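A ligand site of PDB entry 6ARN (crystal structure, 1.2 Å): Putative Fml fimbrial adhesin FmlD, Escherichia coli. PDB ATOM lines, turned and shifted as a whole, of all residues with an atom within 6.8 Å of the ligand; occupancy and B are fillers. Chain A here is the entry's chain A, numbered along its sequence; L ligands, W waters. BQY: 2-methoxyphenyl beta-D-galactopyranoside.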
ATOM      1  N   PHE A   1     -12.952 -29.581   3.563  1.00  0.00           N
ATOM      2  CA  PHE A   1     -13.409 -29.972   4.894  1.00  0.00           C
ATOM      3  C   PHE A   1     -12.908 -31.366   5.193  1.00  0.00           C
ATOM      4  O   PHE A   1     -13.046 -32.266   4.363  1.00  0.00           O
ATOM      5  CB  PHE A   1     -14.928 -29.929   4.977  1.00  0.00           C
ATOM      6  CG  PHE A   1     -15.479 -30.395   6.289  1.00  0.00           C
ATOM      7  CD1 PHE A   1     -16.028 -31.669   6.431  1.00  0.00           C
ATOM      8  CD2 PHE A   1     -15.441 -29.568   7.402  1.00  0.00           C
ATOM      9  CE1 PHE A   1     -16.529 -32.097   7.639  1.00  0.00           C
ATOM     10  CE2 PHE A   1     -15.938 -29.997   8.623  1.00  0.00           C
ATOM     11  CZ  PHE A   1     -16.497 -31.256   8.733  1.00  0.00           C
ATOM     12  N   SER A   2     -12.335 -31.565   6.372  1.00  0.00           N
ATOM     13  CA  SER A   2     -11.810 -32.859   6.747  1.00  0.00           C
ATOM     14  C   SER A   2     -12.030 -33.120   8.235  1.00  0.00           C
ATOM     15  O   SER A   2     -12.181 -32.188   9.025  1.00  0.00           O
ATOM     16  CB  SER A   2     -10.324 -32.961   6.438  1.00  0.00           C
ATOM     17  OG  SER A   2     -10.048 -32.692   5.074  1.00  0.00           O
ATOM     18  N   SER A  10      -6.639 -37.964   7.785  1.00  0.00           N
ATOM     19  CA  SER A  10      -7.767 -37.127   7.373  1.00  0.00           C
ATOM     20  C   SER A  10      -8.855 -37.917   6.652  1.00  0.00           C
ATOM     21  O   SER A  10      -8.577 -38.867   5.929  1.00  0.00           O
ATOM     22  CB  SER A  10      -7.287 -35.980   6.491  1.00  0.00           C
ATOM     23  OG  SER A  10      -6.503 -35.073   7.261  1.00  0.00           O
ATOM     24  N   GLY A  12     -12.415 -37.291   4.307  1.00  0.00           N
ATOM     25  CA  GLY A  12     -13.169 -36.325   3.536  1.00  0.00           C
ATOM     26  C   GLY A  12     -14.609 -36.707   3.271  1.00  0.00           C
ATOM     27  O   GLY A  12     -15.384 -35.890   2.786  1.00  0.00           O
ATOM     28  N   TRP A  43     -12.165 -29.858  10.616  1.00  0.00           N
ATOM     29  CA  TRP A  43     -11.588 -28.538  10.340  1.00  0.00           C
ATOM     30  C   TRP A  43     -11.860 -28.085   8.915  1.00  0.00           C
ATOM     31  O   TRP A  43     -12.216 -28.881   8.029  1.00  0.00           O
ATOM     32  CB  TRP A  43     -10.070 -28.523  10.617  1.00  0.00           C
ATOM     33  CG  TRP A  43      -9.317 -29.510   9.800  1.00  0.00           C
ATOM     34  CD1 TRP A  43      -8.734 -29.308   8.586  1.00  0.00           C
ATOM     35  CD2 TRP A  43      -9.088 -30.894  10.127  1.00  0.00           C
ATOM     36  NE1 TRP A  43      -8.145 -30.469   8.140  1.00  0.00           N
ATOM     37  CE2 TRP A  43      -8.354 -31.455   9.064  1.00  0.00           C
ATOM     38  CE3 TRP A  43      -9.423 -31.704  11.217  1.00  0.00           C
ATOM     39  CZ2 TRP A  43      -7.958 -32.795   9.058  1.00  0.00           C
ATOM     40  CZ3 TRP A  43      -9.030 -33.031  11.206  1.00  0.00           C
ATOM     41  CH2 TRP A  43      -8.303 -33.558  10.134  1.00  0.00           C
ATOM     42  N   ASN A  44     -11.710 -26.790   8.719  1.00  0.00           N
ATOM     43  CA  ASN A  44     -11.793 -26.189   7.415  1.00  0.00           C
ATOM     44  C   ASN A  44     -10.418 -26.311   6.759  1.00  0.00           C
ATOM     45  O   ASN A  44      -9.405 -26.047   7.402  1.00  0.00           O
ATOM     46  CB  ASN A  44     -12.178 -24.722   7.580  1.00  0.00           C
ATOM     47  CG  ASN A  44     -12.395 -24.031   6.272  1.00  0.00           C
ATOM     48  OD1 ASN A  44     -11.445 -23.698   5.582  1.00  0.00           O
ATOM     49  ND2 ASN A  44     -13.662 -23.813   5.922  1.00  0.00           N
ATOM     50  N   ASP A  45     -10.381 -26.707   5.489  1.00  0.00           N
ATOM     51  CA  ASP A  45      -9.103 -27.019   4.870  1.00  0.00           C
ATOM     52  C   ASP A  45      -8.336 -25.803   4.361  1.00  0.00           C
ATOM     53  O   ASP A  45      -7.166 -25.924   4.009  1.00  0.00           O
ATOM     54  CB  ASP A  45      -9.268 -28.068   3.765  1.00  0.00           C
ATOM     55  CG  ASP A  45      -9.317 -29.482   4.313  1.00  0.00           C
ATOM     56  OD1 ASP A  45      -8.330 -29.925   4.934  1.00  0.00           O
ATOM     57  OD2 ASP A  45     -10.345 -30.156   4.117  1.00  0.00           O
ATOM     58  N   TYR A  46      -8.977 -24.627   4.345  1.00  0.00           N
ATOM     59  CA  TYR A  46      -8.277 -23.383   4.043  1.00  0.00           C
ATOM     60  C   TYR A  46      -7.952 -22.583   5.293  1.00  0.00           C
ATOM     61  O   TYR A  46      -6.898 -21.948   5.394  1.00  0.00           O
ATOM     62  CB  TYR A  46      -9.126 -22.484   3.148  1.00  0.00           C
ATOM     63  CG  TYR A  46      -9.486 -23.061   1.811  1.00  0.00           C
ATOM     64  CD1 TYR A  46      -8.504 -23.477   0.917  1.00  0.00           C
ATOM     65  CD2 TYR A  46     -10.817 -23.131   1.411  1.00  0.00           C
ATOM     66  CE1 TYR A  46      -8.852 -23.993  -0.321  1.00  0.00           C
ATOM     67  CE2 TYR A  46     -11.166 -23.640   0.189  1.00  0.00           C
ATOM     68  CZ  TYR A  46     -10.185 -24.067  -0.676  1.00  0.00           C
ATOM     69  OH  TYR A  46     -10.555 -24.574  -1.905  1.00  0.00           O
ATOM     70  N   GLY A  47      -8.872 -22.606   6.251  1.00  0.00           N
ATOM     71  CA  GLY A  47      -8.821 -21.703   7.374  1.00  0.00           C
ATOM     72  C   GLY A  47      -9.240 -20.297   6.958  1.00  0.00           C
ATOM     73  O   GLY A  47      -9.559 -20.049   5.800  1.00  0.00           O
ATOM     74  N   ASP A  51     -13.947 -20.172   2.790  1.00  0.00           N
ATOM     75  CA  ASP A  51     -15.019 -21.010   2.255  1.00  0.00           C
ATOM     76  C   ASP A  51     -15.536 -21.825   3.438  1.00  0.00           C
ATOM     77  O   ASP A  51     -15.057 -22.919   3.699  1.00  0.00           O
ATOM     78  CB  ASP A  51     -14.482 -21.917   1.152  1.00  0.00           C
ATOM     79  CG  ASP A  51     -15.561 -22.727   0.471  1.00  0.00           C
ATOM     80  OD1 ASP A  51     -16.752 -22.477   0.753  1.00  0.00           O
ATOM     81  OD2 ASP A  51     -15.214 -23.591  -0.358  1.00  0.00           O
ATOM     82  N   THR A  52     -16.490 -21.258   4.172  1.00  0.00           N
ATOM     83  CA  THR A  52     -16.904 -21.824   5.449  1.00  0.00           C
ATOM     84  C   THR A  52     -17.699 -23.113   5.277  1.00  0.00           C
ATOM     85  O   THR A  52     -18.563 -23.215   4.395  1.00  0.00           O
ATOM     86  CB  THR A  52     -17.718 -20.800   6.262  1.00  0.00           C
ATOM     87  OG1 THR A  52     -16.891 -19.663   6.558  1.00  0.00           O
ATOM     88  CG2 THR A  52     -18.209 -21.409   7.569  1.00  0.00           C
ATOM     89  N   ASP A  53     -17.400 -24.106   6.114  1.00  0.00           N
ATOM     90  CA  ASP A  53     -18.131 -25.370   6.102  1.00  0.00           C
ATOM     91  C   ASP A  53     -19.332 -25.337   7.035  1.00  0.00           C
ATOM     92  O   ASP A  53     -19.289 -24.750   8.115  1.00  0.00           O
ATOM     93  CB  ASP A  53     -17.208 -26.519   6.465  1.00  0.00           C
ATOM     94  CG  ASP A  53     -16.081 -26.674   5.471  1.00  0.00           C
ATOM     95  OD1 ASP A  53     -16.384 -26.876   4.278  1.00  0.00           O
ATOM     96  OD2 ASP A  53     -14.890 -26.566   5.871  1.00  0.00           O
ATOM     97  N   ILE A  94     -17.820 -24.275  10.455  1.00  0.00           N
ATOM     98  CA  ILE A  94     -16.420 -24.583  10.651  1.00  0.00           C
ATOM     99  C   ILE A  94     -15.588 -23.831   9.622  1.00  0.00           C
ATOM    100  O   ILE A  94     -15.712 -24.055   8.418  1.00  0.00           O
ATOM    101  CB  ILE A  94     -16.184 -26.106  10.540  1.00  0.00           C
ATOM    102  CG1 ILE A  94     -16.931 -26.818  11.686  1.00  0.00           C
ATOM    103  CG2 ILE A  94     -14.700 -26.443  10.524  1.00  0.00           C
ATOM    104  CD1 ILE A  94     -16.486 -28.235  11.949  1.00  0.00           C
ATOM    105  N   LYS A  97      -8.686 -23.699  10.501  1.00  0.00           N
ATOM    106  CA  LYS A  97      -7.911 -24.887  10.152  1.00  0.00           C
ATOM    107  C   LYS A  97      -7.575 -25.697  11.408  1.00  0.00           C
ATOM    108  O   LYS A  97      -7.351 -26.908  11.354  1.00  0.00           O
ATOM    109  CB  LYS A  97      -6.624 -24.485   9.420  1.00  0.00           C
ATOM    110  CG  LYS A  97      -5.722 -25.645   9.030  1.00  0.00           C
ATOM    111  CD  LYS A  97      -6.122 -26.231   7.683  1.00  0.00           C
ATOM    112  CE  LYS A  97      -5.251 -27.440   7.314  1.00  0.00           C
ATOM    113  NZ  LYS A  97      -5.725 -28.111   6.061  1.00  0.00           N
ATOM    114  N   LYS A 132     -22.076 -32.377   5.281  1.00  0.00           N
ATOM    115  CA  LYS A 132     -21.278 -31.186   5.074  1.00  0.00           C
ATOM    116  C   LYS A 132     -21.598 -30.498   3.734  1.00  0.00           C
ATOM    117  O   LYS A 132     -21.705 -31.132   2.724  1.00  0.00           O
ATOM    118  CB  LYS A 132     -19.787 -31.566   5.014  1.00  0.00           C
ATOM    119  CG  LYS A 132     -18.855 -30.427   4.529  1.00  0.00           C
ATOM    120  CD  LYS A 132     -18.376 -30.635   3.071  1.00  0.00           C
ATOM    121  CE  LYS A 132     -17.788 -29.359   2.449  1.00  0.00           C
ATOM    122  NZ  LYS A 132     -17.022 -29.660   1.191  1.00  0.00           N
ATOM    123  N   ILE A 133     -21.701 -29.192   3.792  1.00  0.00           N
ATOM    124  CA  ILE A 133     -21.851 -28.366   2.609  1.00  0.00           C
ATOM    125  C   ILE A 133     -21.129 -27.062   2.906  1.00  0.00           C
ATOM    126  O   ILE A 133     -21.251 -26.541   3.954  1.00  0.00           O
ATOM    127  CB  ILE A 133     -23.287 -28.218   2.116  1.00  0.00           C
ATOM    128  CG1 ILE A 133     -23.312 -27.582   0.698  1.00  0.00           C
ATOM    129  CG2 ILE A 133     -24.148 -27.400   3.075  1.00  0.00           C
ATOM    130  CD1 ILE A 133     -24.690 -27.550   0.068  1.00  0.00           C
ATOM    131  N   ALA A 134     -20.327 -26.606   1.956  1.00  0.00           N
ATOM    132  CA  ALA A 134     -19.575 -25.381   2.137  1.00  0.00           C
ATOM    133  C   ALA A 134     -20.322 -24.183   1.642  1.00  0.00           C
ATOM    134  O   ALA A 134     -21.482 -24.197   1.549  1.00  0.00           O
ATOM    135  CB  ALA A 134     -18.151 -25.505   1.584  1.00  0.00           C
ATOM    136  N   THR A 135     -19.592 -23.106   1.320  1.00  0.00           N
ATOM    137  CA  THR A 135     -20.151 -21.821   0.986  1.00  0.00           C
ATOM    138  C   THR A 135     -20.001 -21.406  -0.469  1.00  0.00           C
ATOM    139  O   THR A 135     -20.903 -20.863  -1.012  1.00  0.00           O
ATOM    140  CB  THR A 135     -19.484 -20.749   1.896  1.00  0.00           C
ATOM    141  OG1 THR A 135     -19.677 -21.138   3.264  1.00  0.00           O
ATOM    142  CG2 THR A 135     -20.065 -19.329   1.749  1.00  0.00           C
ATOM    143  N   LEU A 136     -18.848 -21.677  -1.033  1.00  0.00           N
ATOM    144  CA  LEU A 136     -18.573 -21.260  -2.412  1.00  0.00           C
ATOM    145  C   LEU A 136     -19.026 -22.321  -3.410  1.00  0.00           C
ATOM    146  O   LEU A 136     -19.082 -23.511  -3.093  1.00  0.00           O
ATOM    147  CB  LEU A 136     -17.090 -20.969  -2.592  1.00  0.00           C
ATOM    148  CG  LEU A 136     -16.530 -19.862  -1.694  1.00  0.00           C
ATOM    149  CD1 LEU A 136     -15.039 -19.688  -1.910  1.00  0.00           C
ATOM    150  CD2 LEU A 136     -17.273 -18.547  -1.893  1.00  0.00           C
ATOM    151  N   GLY A 139     -20.907 -25.801  -2.989  1.00  0.00           N
ATOM    152  CA  GLY A 139     -20.662 -26.172  -1.614  1.00  0.00           C
ATOM    153  C   GLY A 139     -20.026 -27.533  -1.473  1.00  0.00           C
ATOM    154  O   GLY A 139     -19.674 -27.939  -0.364  1.00  0.00           O
ATOM    155  N   ASN A 140     -19.879 -28.260  -2.588  1.00  0.00           N
ATOM    156  CA  ASN A 140     -19.224 -29.567  -2.590  1.00  0.00           C
ATOM    157  C   ASN A 140     -19.693 -30.452  -1.438  1.00  0.00           C
ATOM    158  O   ASN A 140     -18.906 -30.836  -0.576  1.00  0.00           O
ATOM    159  CB  ASN A 140     -17.707 -29.418  -2.555  1.00  0.00           C
ATOM    160  CG  ASN A 140     -17.184 -28.617  -3.719  1.00  0.00           C
ATOM    161  OD1 ASN A 140     -17.876 -28.457  -4.726  1.00  0.00           O
ATOM    162  ND2 ASN A 140     -15.962 -28.116  -3.600  1.00  0.00           N
ATOM    163  N   PRO A 141     -20.987 -30.781  -1.432  1.00  0.00           N
ATOM    164  CA  PRO A 141     -21.564 -31.550  -0.321  1.00  0.00           C
ATOM    165  C   PRO A 141     -20.946 -32.928  -0.160  1.00  0.00           C
ATOM    166  O   PRO A 141     -20.589 -33.584  -1.138  1.00  0.00           O
ATOM    167  CB  PRO A 141     -23.045 -31.678  -0.705  1.00  0.00           C
ATOM    168  CG  PRO A 141     -23.072 -31.480  -2.195  1.00  0.00           C
ATOM    169  CD  PRO A 141     -21.987 -30.481  -2.476  1.00  0.00           C
ATOM    170  N   ARG A 142     -20.812 -33.365   1.097  1.00  0.00           N
ATOM    171  CA  ARG A 142     -20.225 -34.650   1.406  1.00  0.00           C
ATOM    172  C   ARG A 142     -20.985 -35.320   2.545  1.00  0.00           C
ATOM    173  O   ARG A 142     -21.506 -34.652   3.439  1.00  0.00           O
ATOM    174  CB  ARG A 142     -18.772 -34.484   1.848  1.00  0.00           C
ATOM    175  CG  ARG A 142     -17.846 -33.876   0.803  1.00  0.00           C
ATOM    176  CD  ARG A 142     -17.455 -34.897  -0.253  1.00  0.00           C
ATOM    177  NE  ARG A 142     -16.434 -34.371  -1.159  1.00  0.00           N
ATOM    178  CZ  ARG A 142     -15.128 -34.498  -0.950  1.00  0.00           C
ATOM    179  NH1 ARG A 142     -14.678 -35.124   0.126  1.00  0.00           N
ATOM    180  NH2 ARG A 142     -14.264 -33.989  -1.833  1.00  0.00           N
HETATM  181  C10 BQY L   1      -7.184 -28.154   0.752  1.00  0.00           C
HETATM  182  C2  BQY L   1     -13.577 -28.180  -0.189  1.00  0.00           C
HETATM  183  C3  BQY L   1     -14.570 -27.073   0.002  1.00  0.00           C
HETATM  184  O6  BQY L   1     -12.988 -26.706   4.134  1.00  0.00           O
HETATM  185  C6  BQY L   1     -12.958 -25.661   3.218  1.00  0.00           C
HETATM  186  C5  BQY L   1     -13.098 -26.219   1.776  1.00  0.00           C
HETATM  187  O5  BQY L   1     -12.252 -27.291   1.617  1.00  0.00           O
HETATM  188  C1  BQY L   1     -12.201 -27.720   0.286  1.00  0.00           C
HETATM  189  O1  BQY L   1     -11.331 -28.836   0.198  1.00  0.00           O
HETATM  190  C07 BQY L   1      -9.920 -28.545   0.389  1.00  0.00           C
HETATM  191  C08 BQY L   1      -9.402 -27.252   0.402  1.00  0.00           C
HETATM  192  C09 BQY L   1      -8.026 -27.053   0.589  1.00  0.00           C
HETATM  193  C11 BQY L   1      -7.698 -29.442   0.730  1.00  0.00           C
HETATM  194  C12 BQY L   1      -9.067 -29.638   0.549  1.00  0.00           C
HETATM  195  O13 BQY L   1      -9.638 -30.935   0.523  1.00  0.00           O
HETATM  196  C14 BQY L   1      -9.103 -31.850   1.451  1.00  0.00           C
HETATM  197  O2  BQY L   1     -13.518 -28.509  -1.558  1.00  0.00           O
HETATM  198  O3  BQY L   1     -15.864 -27.544  -0.397  1.00  0.00           O
HETATM  199  C4  BQY L   1     -14.527 -26.645   1.443  1.00  0.00           C
HETATM  200  O4  BQY L   1     -14.951 -27.724   2.252  1.00  0.00           O
HETATM  201  O   HOH W   1     -12.556 -31.547   0.134  1.00  0.00           O
HETATM  202  O   HOH W   2     -16.940 -25.281  -1.629  1.00  0.00           O
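An oxygen (O6) of the ligand lies within hydrogen-bond range of the side-chain carboxylate (OD2) of Asp 53, 2.6 Å away. An oxygen (O3) of the ligand is in hydrogen-bond range of the side-chain amino group (NZ) of Lys 132, at 2.9 Å. The backbone NH of Phe 1 is in hydrogen-bond range of an oxygen (O6) of the ligand. O6 of the ligand is in hydrogen-bond range of N of Asp 45, 2.9 Å away. The side-chain amide nitrogen of Asn 140 lies within hydrogen-bond range of an oxygen (O2) of the ligand (3.2 Å). An oxygen (O6) of the ligand sits close to the side-chain amide nitrogen (ND2) of Asn 44 (3.5 Å).
The side-chain amide nitrogen (ND2) of Asn 44 is in hydrogen-bond range of the side-chain carboxylate (OD2) of Asp 53. The backbone carbonyl oxygen (O) of Asp 53 lies within hydrogen-bond range of the backbone NH (N) of Ile 94 (2.8 Å). The side-chain amino group (NZ) of Lys 132 is in hydrogen-bond range of the backbone carbonyl oxygen (O) of Asn 140. O of Lys 132 sits at hydrogen-bond distance from N of Arg 142, 2.9 Å away. OD2 of Asp 45 sits at hydrogen-bond distance from N of Phe 1. The side-chain carboxylate (OD1) of Asp 45 lies within salt-bridge range of the side-chain amino group (NZ) of Lys 97, 3.4 Å away. The backbone carbonyl oxygen (O) of Ile 94 sits at hydrogen-bond distance from the side-chain amide nitrogen (ND2) of Asn 44, at 3.2 Å. The backbone carbonyl oxygen (O) of Gly 139 lies within hydrogen-bond range of the backbone NH (N) of Ala 134, 2.8 Å away.
Water W2 lies within hydrogen-bond range of the side-chain carboxylate (OD2) of Asp 51, an oxygen (O3) of the ligand and the backbone carbonyl oxygen (O) of Leu 136.
Ser 2 touches the ligand (OG to C14, 3.8 Å). CE1 of Tyr 46 touches C09 of the ligand, 3.3 Å away. O of Asp 51 touches C6 of the ligand, at 3.5 Å. CB of Ala 134 touches O3 of the ligand, 3.6 Å away. Gly 139 touches the ligand. 11 residues have an atom within 4 Å of the ligand: Phe 1, Ser 2, Asn 44, Asp 45, Tyr 46, Asp 51, Asp 53, Lys 132, Ala 134, Gly 139 and Asn 140.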
